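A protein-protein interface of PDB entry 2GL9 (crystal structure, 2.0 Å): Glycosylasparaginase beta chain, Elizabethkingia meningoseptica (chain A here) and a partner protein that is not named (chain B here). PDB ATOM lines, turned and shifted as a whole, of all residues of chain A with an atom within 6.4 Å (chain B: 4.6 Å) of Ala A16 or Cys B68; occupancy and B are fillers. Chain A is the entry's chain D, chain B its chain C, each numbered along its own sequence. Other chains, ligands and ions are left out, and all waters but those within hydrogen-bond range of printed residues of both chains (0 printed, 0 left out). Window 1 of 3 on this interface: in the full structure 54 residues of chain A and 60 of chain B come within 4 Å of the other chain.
The backbone carbonyl oxygen of Pro A34 sits at hydrogen-bond distance from the side-chain hydroxyl of Ser B78 (3.0 Å).
The backbone carbonyl oxygen (O) of Ser A33 sits at hydrogen-bond distance from the side-chain sulfur (SG) of Cys B68 (3.2 Å).
SD of Met B70 lies within hydrogen-bond range of N of Val A42 (3.4 Å).
The backbone NH (N) of Cys B68 sits at hydrogen-bond distance from the backbone carbonyl oxygen (O) of Cys A17.
The backbone carbonyl oxygen (O) of Met B70 is in hydrogen-bond range of the backbone NH (N) of Gly A15, at 3.0 Å.
The backbone NH (N) of Met A4 sits at hydrogen-bond distance from the backbone carbonyl oxygen (O) of Ala A16.
N of Ile B69 is in hydrogen-bond range of O of Gly B77 (2.8 Å).
O of Ser A33 lies close to SG of Cys A17, 3.5 Å away.
The backbone carbonyl oxygen of Thr A18 lies within hydrogen-bond range of the backbone NH of Ile A2, 3.0 Å away.
Among the printed residues, pairs that only touch across the chains: Cys A17 with Ala B67 (3.1 Å), Ser A14 with Met B70 (3.3 Å), Gly A15 with Ile B69 (3.4 Å), Ala A16 with Ile B89 (3.5 Å), Ala A16 with Cys B68 (3.5 Å), Pro A34 with Cys B68 (3.5 Å), Thr A18 with Val B39 (3.6 Å), Pro A34 with Ala B67 (3.7 Å), Met A4 with Val B35 (3.7 Å), Gly A15 with Val B35 (3.7 Å), Ala A16 with Val B35 (3.7 Å), Thr A18 with Ala B67 (3.8 Å), Ile A2 with Val B39 (3.8 Å), Ile A36 with Cys B68 (3.8 Å), Leu A40 with Cys B68 (3.8 Å), Ser A14 with Val B35 (3.8 Å), Met A4 with Val B39 (3.8 Å), Cys A17 with Ile B89 (3.9 Å), Leu A40 with Met B70 (3.97 Å), Ala A16 with Val B39 (3.97 Å) and Ile A36 with Met B70 (3.99 Å).
Ala A16 touches just these residues of chain B: Val B35 (3.7 Å), Val B39 (3.97 Å), Cys B68 (3.5 Å) and Ile B89 (3.5 Å).
Of chain A, only Ala A16, Cys A17, Ser A33, Pro A34, Ile A36 and Leu A40 come within 4 Å of Cys B68.
Of the printed residues of chain B, Met A4 touches Val B35 (3.7 Å) and Val B39 (3.8 Å).
Of the printed residues of chain B, Ser A14 touches Val B35 and Met B70.
Of the printed residues of chain B, Cys A17 touches Ala B67, Cys B68 and Ile B89.
Glu B36 touches none of the printed residues of chain A.
The nearest residue of chain B that does not touch Ala A16 is Ile B69 (4.4 Å).
The nearest residue of chain A that does not touch Cys B68 is Ile A35 (4.2 Å).
The nearest printed residue of chain B that does not touch Leu A40 is Ile B69 (4.1 Å).
Hydrophobic or aromatic side chains of chain A that line the printed part of chain B: Ile A2, Met A4, Ala A16, Pro A34, Ile A36, Leu A40 and Val A42.
Of the 11 printed residues of chain B, 8 touch a printed residue of chain A.
Printed residues of chain B that touch a printed residue of chain A: Val B35, Val B39, Ala B67, Cys B68, Ile B69, Met B70, Ser B78 and Ile B89.
Hydrophobic or aromatic side chains of chain B within 4 Å of the printed part of chain A: Val B35, Val B39, Ala B67, Ile B69, Met B70 and Ile B89.
Among the printed residues, 26 pairs touch across the chains.
Among the printed residues, no Asp or Glu carboxylate lies within 4 Å of a Lys or Arg side-chain nitrogen of the other chain.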
ATOM      1  N   ILE A   2       4.840  -7.303  -2.879  1.00  0.00           N
ATOM      2  CA  ILE A   2       5.475  -8.012  -3.963  1.00  0.00           C
ATOM      3  C   ILE A   2       4.608  -7.614  -5.147  1.00  0.00           C
ATOM      4  O   ILE A   2       3.374  -7.667  -5.053  1.00  0.00           O
ATOM      5  CB  ILE A   2       5.514  -9.572  -3.826  1.00  0.00           C
ATOM      6  CG1 ILE A   2       6.129 -10.158  -5.123  1.00  0.00           C
ATOM      7  CG2 ILE A   2       4.127 -10.140  -3.555  1.00  0.00           C
ATOM      8  CD1 ILE A   2       6.372 -11.667  -5.114  1.00  0.00           C
ATOM      9  N   GLY A   3       5.252  -7.147  -6.216  1.00  0.00           N
ATOM     10  CA  GLY A   3       4.531  -6.782  -7.433  1.00  0.00           C
ATOM     11  C   GLY A   3       5.060  -7.729  -8.509  1.00  0.00           C
ATOM     12  O   GLY A   3       6.281  -8.011  -8.557  1.00  0.00           O
ATOM     13  N   MET A   4       4.171  -8.223  -9.380  1.00  0.00           N
ATOM     14  CA  MET A   4       4.583  -9.165 -10.405  1.00  0.00           C
ATOM     15  C   MET A   4       3.851  -8.902 -11.706  1.00  0.00           C
ATOM     16  O   MET A   4       2.615  -8.757 -11.728  1.00  0.00           O
ATOM     17  CB  MET A   4       4.292 -10.601  -9.929  1.00  0.00           C
ATOM     18  CG  MET A   4       4.843 -11.670 -10.865  1.00  0.00           C
ATOM     19  SD  MET A   4       4.496 -13.369 -10.266  1.00  0.00           S
ATOM     20  CE  MET A   4       5.991 -13.600  -9.116  1.00  0.00           C
ATOM     21  N   ILE A   5       4.616  -8.849 -12.786  1.00  0.00           N
ATOM     22  CA  ILE A   5       4.041  -8.602 -14.092  1.00  0.00           C
ATOM     23  C   ILE A   5       4.576  -9.668 -15.019  1.00  0.00           C
ATOM     24  O   ILE A   5       5.726 -10.127 -14.865  1.00  0.00           O
ATOM     25  CB  ILE A   5       4.401  -7.189 -14.600  1.00  0.00           C
ATOM     26  CG1 ILE A   5       5.923  -6.948 -14.501  1.00  0.00           C
ATOM     27  CG2 ILE A   5       3.640  -6.149 -13.759  1.00  0.00           C
ATOM     28  CD1 ILE A   5       6.394  -5.549 -15.041  1.00  0.00           C
ATOM     29  N   SER A  14      -0.362  -9.211 -17.794  1.00  0.00           N
ATOM     30  CA  SER A  14      -1.180  -9.156 -16.550  1.00  0.00           C
ATOM     31  C   SER A  14      -0.230  -8.845 -15.384  1.00  0.00           C
ATOM     32  O   SER A  14       0.991  -8.968 -15.520  1.00  0.00           O
ATOM     33  CB  SER A  14      -1.909 -10.470 -16.266  1.00  0.00           C
ATOM     34  OG  SER A  14      -2.983 -10.642 -17.173  1.00  0.00           O
ATOM     35  N   GLY A  15      -0.786  -8.432 -14.249  1.00  0.00           N
ATOM     36  CA  GLY A  15       0.044  -8.113 -13.115  1.00  0.00           C
ATOM     37  C   GLY A  15      -0.759  -8.224 -11.838  1.00  0.00           C
ATOM     38  O   GLY A  15      -2.001  -8.181 -11.845  1.00  0.00           O
ATOM     39  N   ALA A  16      -0.023  -8.324 -10.740  1.00  0.00           N
ATOM     40  CA  ALA A  16      -0.584  -8.477  -9.425  1.00  0.00           C
ATOM     41  C   ALA A  16       0.321  -7.741  -8.450  1.00  0.00           C
ATOM     42  O   ALA A  16       1.542  -7.689  -8.624  1.00  0.00           O
ATOM     43  CB  ALA A  16      -0.634  -9.979  -9.055  1.00  0.00           C
ATOM     44  N   CYS A  17      -0.279  -7.209  -7.398  1.00  0.00           N
ATOM     45  CA  CYS A  17       0.455  -6.461  -6.405  1.00  0.00           C
ATOM     46  C   CYS A  17      -0.244  -6.743  -5.069  1.00  0.00           C
ATOM     47  O   CYS A  17      -1.464  -6.644  -4.974  1.00  0.00           O
ATOM     48  CB  CYS A  17       0.444  -4.974  -6.795  1.00  0.00           C
ATOM     49  SG  CYS A  17       1.532  -3.958  -5.773  1.00  0.00           S
ATOM     50  N   THR A  18       0.520  -7.135  -4.044  1.00  0.00           N
ATOM     51  CA  THR A  18      -0.073  -7.470  -2.737  1.00  0.00           C
ATOM     52  C   THR A  18       0.904  -7.148  -1.617  1.00  0.00           C
ATOM     53  O   THR A  18       2.104  -7.403  -1.740  1.00  0.00           O
ATOM     54  CB  THR A  18      -0.518  -8.995  -2.697  1.00  0.00           C
ATOM     55  OG1 THR A  18      -1.069  -9.308  -1.417  1.00  0.00           O
ATOM     56  CG2 THR A  18       0.628  -9.939  -2.996  1.00  0.00           C
ATOM     57  N   ASP A  32       0.216   2.438  -2.198  1.00  0.00           N
ATOM     58  CA  ASP A  32      -0.004   2.341  -3.638  1.00  0.00           C
ATOM     59  C   ASP A  32      -0.371   0.952  -4.143  1.00  0.00           C
ATOM     60  O   ASP A  32      -0.944   0.816  -5.222  1.00  0.00           O
ATOM     61  CB  ASP A  32       1.269   2.771  -4.359  1.00  0.00           C
ATOM     62  CG  ASP A  32       2.435   1.830  -4.043  1.00  0.00           C
ATOM     63  OD1 ASP A  32       2.548   1.395  -2.872  1.00  0.00           O
ATOM     64  OD2 ASP A  32       3.238   1.496  -4.953  1.00  0.00           O
ATOM     65  N   SER A  33      -0.042  -0.081  -3.377  1.00  0.00           N
ATOM     66  CA  SER A  33      -0.256  -1.443  -3.850  1.00  0.00           C
ATOM     67  C   SER A  33      -1.635  -1.853  -4.359  1.00  0.00           C
ATOM     68  O   SER A  33      -1.726  -2.752  -5.179  1.00  0.00           O
ATOM     69  CB  SER A  33       0.232  -2.441  -2.807  1.00  0.00           C
ATOM     70  OG  SER A  33       1.569  -2.124  -2.439  1.00  0.00           O
ATOM     71  N   PRO A  34      -2.723  -1.234  -3.856  1.00  0.00           N
ATOM     72  CA  PRO A  34      -4.041  -1.631  -4.373  1.00  0.00           C
ATOM     73  C   PRO A  34      -4.570  -0.547  -5.338  1.00  0.00           C
ATOM     74  O   PRO A  34      -5.711  -0.617  -5.802  1.00  0.00           O
ATOM     75  CB  PRO A  34      -4.890  -1.677  -3.108  1.00  0.00           C
ATOM     76  CG  PRO A  34      -4.415  -0.426  -2.428  1.00  0.00           C
ATOM     77  CD  PRO A  34      -2.888  -0.457  -2.615  1.00  0.00           C
ATOM     78  N   ILE A  35      -3.771   0.477  -5.605  1.00  0.00           N
ATOM     79  CA  ILE A  35      -4.263   1.556  -6.471  1.00  0.00           C
ATOM     80  C   ILE A  35      -3.812   1.389  -7.917  1.00  0.00           C
ATOM     81  O   ILE A  35      -2.619   1.441  -8.184  1.00  0.00           O
ATOM     82  CB  ILE A  35      -3.762   2.936  -6.008  1.00  0.00           C
ATOM     83  CG1 ILE A  35      -4.055   3.171  -4.521  1.00  0.00           C
ATOM     84  CG2 ILE A  35      -4.396   4.029  -6.889  1.00  0.00           C
ATOM     85  CD1 ILE A  35      -5.514   2.999  -4.158  1.00  0.00           C
ATOM     86  N   ILE A  36      -4.766   1.218  -8.833  1.00  0.00           N
ATOM     87  CA  ILE A  36      -4.472   1.058 -10.260  1.00  0.00           C
ATOM     88  C   ILE A  36      -3.874   2.376 -10.754  1.00  0.00           C
ATOM     89  O   ILE A  36      -4.403   3.438 -10.497  1.00  0.00           O
ATOM     90  CB  ILE A  36      -5.779   0.717 -11.091  1.00  0.00           C
ATOM     91  CG1 ILE A  36      -6.363  -0.644 -10.655  1.00  0.00           C
ATOM     92  CG2 ILE A  36      -5.461   0.700 -12.620  1.00  0.00           C
ATOM     93  CD1 ILE A  36      -5.378  -1.850 -10.881  1.00  0.00           C
ATOM     94  N   GLY A  39       0.467   1.669  -7.757  1.00  0.00           N
ATOM     95  CA  GLY A  39       1.274   0.467  -7.606  1.00  0.00           C
ATOM     96  C   GLY A  39       1.296  -0.510  -8.781  1.00  0.00           C
ATOM     97  O   GLY A  39       2.221  -1.330  -8.920  1.00  0.00           O
ATOM     98  N   LEU A  40       0.283  -0.448  -9.636  1.00  0.00           N
ATOM     99  CA  LEU A  40       0.227  -1.386 -10.746  1.00  0.00           C
ATOM    100  C   LEU A  40      -0.547  -0.862 -11.929  1.00  0.00           C
ATOM    101  O   LEU A  40      -1.586  -0.241 -11.748  1.00  0.00           O
ATOM    102  CB  LEU A  40      -0.433  -2.703 -10.279  1.00  0.00           C
ATOM    103  CG  LEU A  40      -0.704  -3.758 -11.360  1.00  0.00           C
ATOM    104  CD1 LEU A  40       0.627  -4.276 -11.891  1.00  0.00           C
ATOM    105  CD2 LEU A  40      -1.567  -4.917 -10.840  1.00  0.00           C
ATOM    106  N   VAL A  42      -1.453  -2.067 -16.221  1.00  0.00           N
ATOM    107  CA  VAL A  42      -1.228  -2.937 -17.378  1.00  0.00           C
ATOM    108  C   VAL A  42      -2.057  -2.480 -18.593  1.00  0.00           C
ATOM    109  O   VAL A  42      -3.246  -2.272 -18.476  1.00  0.00           O
ATOM    110  CB  VAL A  42      -1.624  -4.410 -17.066  1.00  0.00           C
ATOM    111  CG1 VAL A  42      -1.483  -5.250 -18.310  1.00  0.00           C
ATOM    112  CG2 VAL A  42      -0.759  -5.000 -15.918  1.00  0.00           C
ATOM    113  N   THR A  50       5.022  -2.139 -12.325  1.00  0.00           N
ATOM    114  CA  THR A  50       4.584  -2.257 -10.959  1.00  0.00           C
ATOM    115  C   THR A  50       5.656  -1.501 -10.170  1.00  0.00           C
ATOM    116  O   THR A  50       6.836  -1.441 -10.575  1.00  0.00           O
ATOM    117  CB  THR A  50       4.357  -3.732 -10.526  1.00  0.00           C
ATOM    118  OG1 THR A  50       3.727  -3.741  -9.236  1.00  0.00           O
ATOM    119  CG2 THR A  50       5.651  -4.523 -10.480  1.00  0.00           C
ATOM    120  N   VAL B  35       0.605 -14.670 -12.447  1.00  0.00           N
ATOM    121  CA  VAL B  35       0.911 -13.627 -11.443  1.00  0.00           C
ATOM    122  C   VAL B  35       0.152 -13.806 -10.163  1.00  0.00           C
ATOM    123  O   VAL B  35       0.660 -13.464  -9.108  1.00  0.00           O
ATOM    124  CB  VAL B  35       0.707 -12.167 -11.970  1.00  0.00           C
ATOM    125  CG1 VAL B  35       1.593 -11.953 -13.200  1.00  0.00           C
ATOM    126  CG2 VAL B  35      -0.800 -11.883 -12.310  1.00  0.00           C
ATOM    127  N   GLU B  36      -1.052 -14.373 -10.235  1.00  0.00           N
ATOM    128  CA  GLU B  36      -1.815 -14.622  -9.009  1.00  0.00           C
ATOM    129  C   GLU B  36      -1.131 -15.728  -8.182  1.00  0.00           C
ATOM    130  O   GLU B  36      -0.925 -15.569  -6.962  1.00  0.00           O
ATOM    131  CB  GLU B  36      -3.250 -15.060  -9.302  1.00  0.00           C
ATOM    132  CG  GLU B  36      -3.988 -15.478  -8.030  1.00  0.00           C
ATOM    133  CD  GLU B  36      -5.431 -15.918  -8.271  1.00  0.00           C
ATOM    134  OE1 GLU B  36      -5.728 -16.479  -9.354  1.00  0.00           O
ATOM    135  OE2 GLU B  36      -6.254 -15.698  -7.366  1.00  0.00           O
ATOM    136  N   VAL B  39       2.313 -14.500  -6.569  1.00  0.00           N
ATOM    137  CA  VAL B  39       2.303 -13.692  -5.346  1.00  0.00           C
ATOM    138  C   VAL B  39       1.633 -14.397  -4.167  1.00  0.00           C
ATOM    139  O   VAL B  39       1.973 -14.116  -3.007  1.00  0.00           O
ATOM    140  CB  VAL B  39       1.694 -12.270  -5.572  1.00  0.00           C
ATOM    141  CG1 VAL B  39       2.522 -11.536  -6.658  1.00  0.00           C
ATOM    142  CG2 VAL B  39       0.226 -12.369  -5.999  1.00  0.00           C
ATOM    143  N   ALA B  67      -4.210  -5.101  -1.986  1.00  0.00           N
ATOM    144  CA  ALA B  67      -3.793  -5.819  -3.176  1.00  0.00           C
ATOM    145  C   ALA B  67      -4.665  -5.441  -4.347  1.00  0.00           C
ATOM    146  O   ALA B  67      -5.832  -5.054  -4.164  1.00  0.00           O
ATOM    147  CB  ALA B  67      -3.895  -7.356  -2.942  1.00  0.00           C
ATOM    148  N   CYS B  68      -4.093  -5.527  -5.550  1.00  0.00           N
ATOM    149  CA  CYS B  68      -4.876  -5.300  -6.753  1.00  0.00           C
ATOM    150  C   CYS B  68      -4.338  -6.171  -7.882  1.00  0.00           C
ATOM    151  O   CYS B  68      -3.176  -6.656  -7.855  1.00  0.00           O
ATOM    152  CB  CYS B  68      -4.938  -3.808  -7.142  1.00  0.00           C
ATOM    153  SG  CYS B  68      -3.469  -3.065  -7.858  1.00  0.00           S
ATOM    154  N   ILE B  69      -5.180  -6.397  -8.871  1.00  0.00           N
ATOM    155  CA  ILE B  69      -4.795  -7.244  -9.986  1.00  0.00           C
ATOM    156  C   ILE B  69      -5.348  -6.603 -11.255  1.00  0.00           C
ATOM    157  O   ILE B  69      -6.355  -5.895 -11.197  1.00  0.00           O
ATOM    158  CB  ILE B  69      -5.386  -8.660  -9.757  1.00  0.00           C
ATOM    159  CG1 ILE B  69      -4.757  -9.696 -10.681  1.00  0.00           C
ATOM    160  CG2 ILE B  69      -6.899  -8.606  -9.898  1.00  0.00           C
ATOM    161  CD1 ILE B  69      -5.075 -11.084 -10.189  1.00  0.00           C
ATOM    162  N   MET B  70      -4.684  -6.821 -12.390  1.00  0.00           N
ATOM    163  CA  MET B  70      -5.164  -6.254 -13.661  1.00  0.00           C
ATOM    164  C   MET B  70      -4.806  -7.222 -14.776  1.00  0.00           C
ATOM    165  O   MET B  70      -3.661  -7.691 -14.843  1.00  0.00           O
ATOM    166  CB  MET B  70      -4.513  -4.884 -13.896  1.00  0.00           C
ATOM    167  CG  MET B  70      -5.024  -4.135 -15.095  1.00  0.00           C
ATOM    168  SD  MET B  70      -4.582  -2.358 -15.025  1.00  0.00           S
ATOM    169  CE  MET B  70      -5.864  -1.690 -16.252  1.00  0.00           C
ATOM    170  N   GLY B  77      -9.262  -5.412 -10.273  1.00  0.00           N
ATOM    171  CA  GLY B  77      -9.849  -5.781  -8.993  1.00  0.00           C
ATOM    172  C   GLY B  77      -8.897  -5.335  -7.899  1.00  0.00           C
ATOM    173  O   GLY B  77      -7.664  -5.457  -8.028  1.00  0.00           O
ATOM    174  N   SER B  78      -9.467  -4.860  -6.797  1.00  0.00           N
ATOM    175  CA  SER B  78      -8.655  -4.341  -5.714  1.00  0.00           C
ATOM    176  C   SER B  78      -9.323  -4.427  -4.353  1.00  0.00           C
ATOM    177  O   SER B  78     -10.531  -4.261  -4.248  1.00  0.00           O
ATOM    178  CB  SER B  78      -8.354  -2.862  -5.985  1.00  0.00           C
ATOM    179  OG  SER B  78      -7.998  -2.203  -4.775  1.00  0.00           O
ATOM    180  N   ILE B  89      -4.850 -11.039  -2.873  1.00  0.00           N
ATOM    181  CA  ILE B  89      -4.778 -10.974  -4.335  1.00  0.00           C
ATOM    182  C   ILE B  89      -5.930 -11.747  -4.979  1.00  0.00           C
ATOM    183  O   ILE B  89      -6.459 -11.323  -6.016  1.00  0.00           O
ATOM    184  CB  ILE B  89      -3.443 -11.476  -4.919  1.00  0.00           C
ATOM    185  CG1 ILE B  89      -3.399 -11.138  -6.420  1.00  0.00           C
ATOM    186  CG2 ILE B  89      -3.263 -13.028  -4.695  1.00  0.00           C
ATOM    187  CD1 ILE B  89      -3.267  -9.647  -6.752  1.00  0.00           C
ATOM    188  N   ALA B  92      -9.078  -9.792  -4.584  1.00  0.00           N
ATOM    189  CA  ALA B  92      -9.092  -8.721  -5.594  1.00  0.00           C
ATOM    190  C   ALA B  92      -9.563  -9.330  -6.912  1.00  0.00           C
ATOM    191  O   ALA B  92     -10.375  -8.741  -7.628  1.00  0.00           O
ATOM    192  CB  ALA B  92      -7.690  -8.089  -5.767  1.00  0.00           C
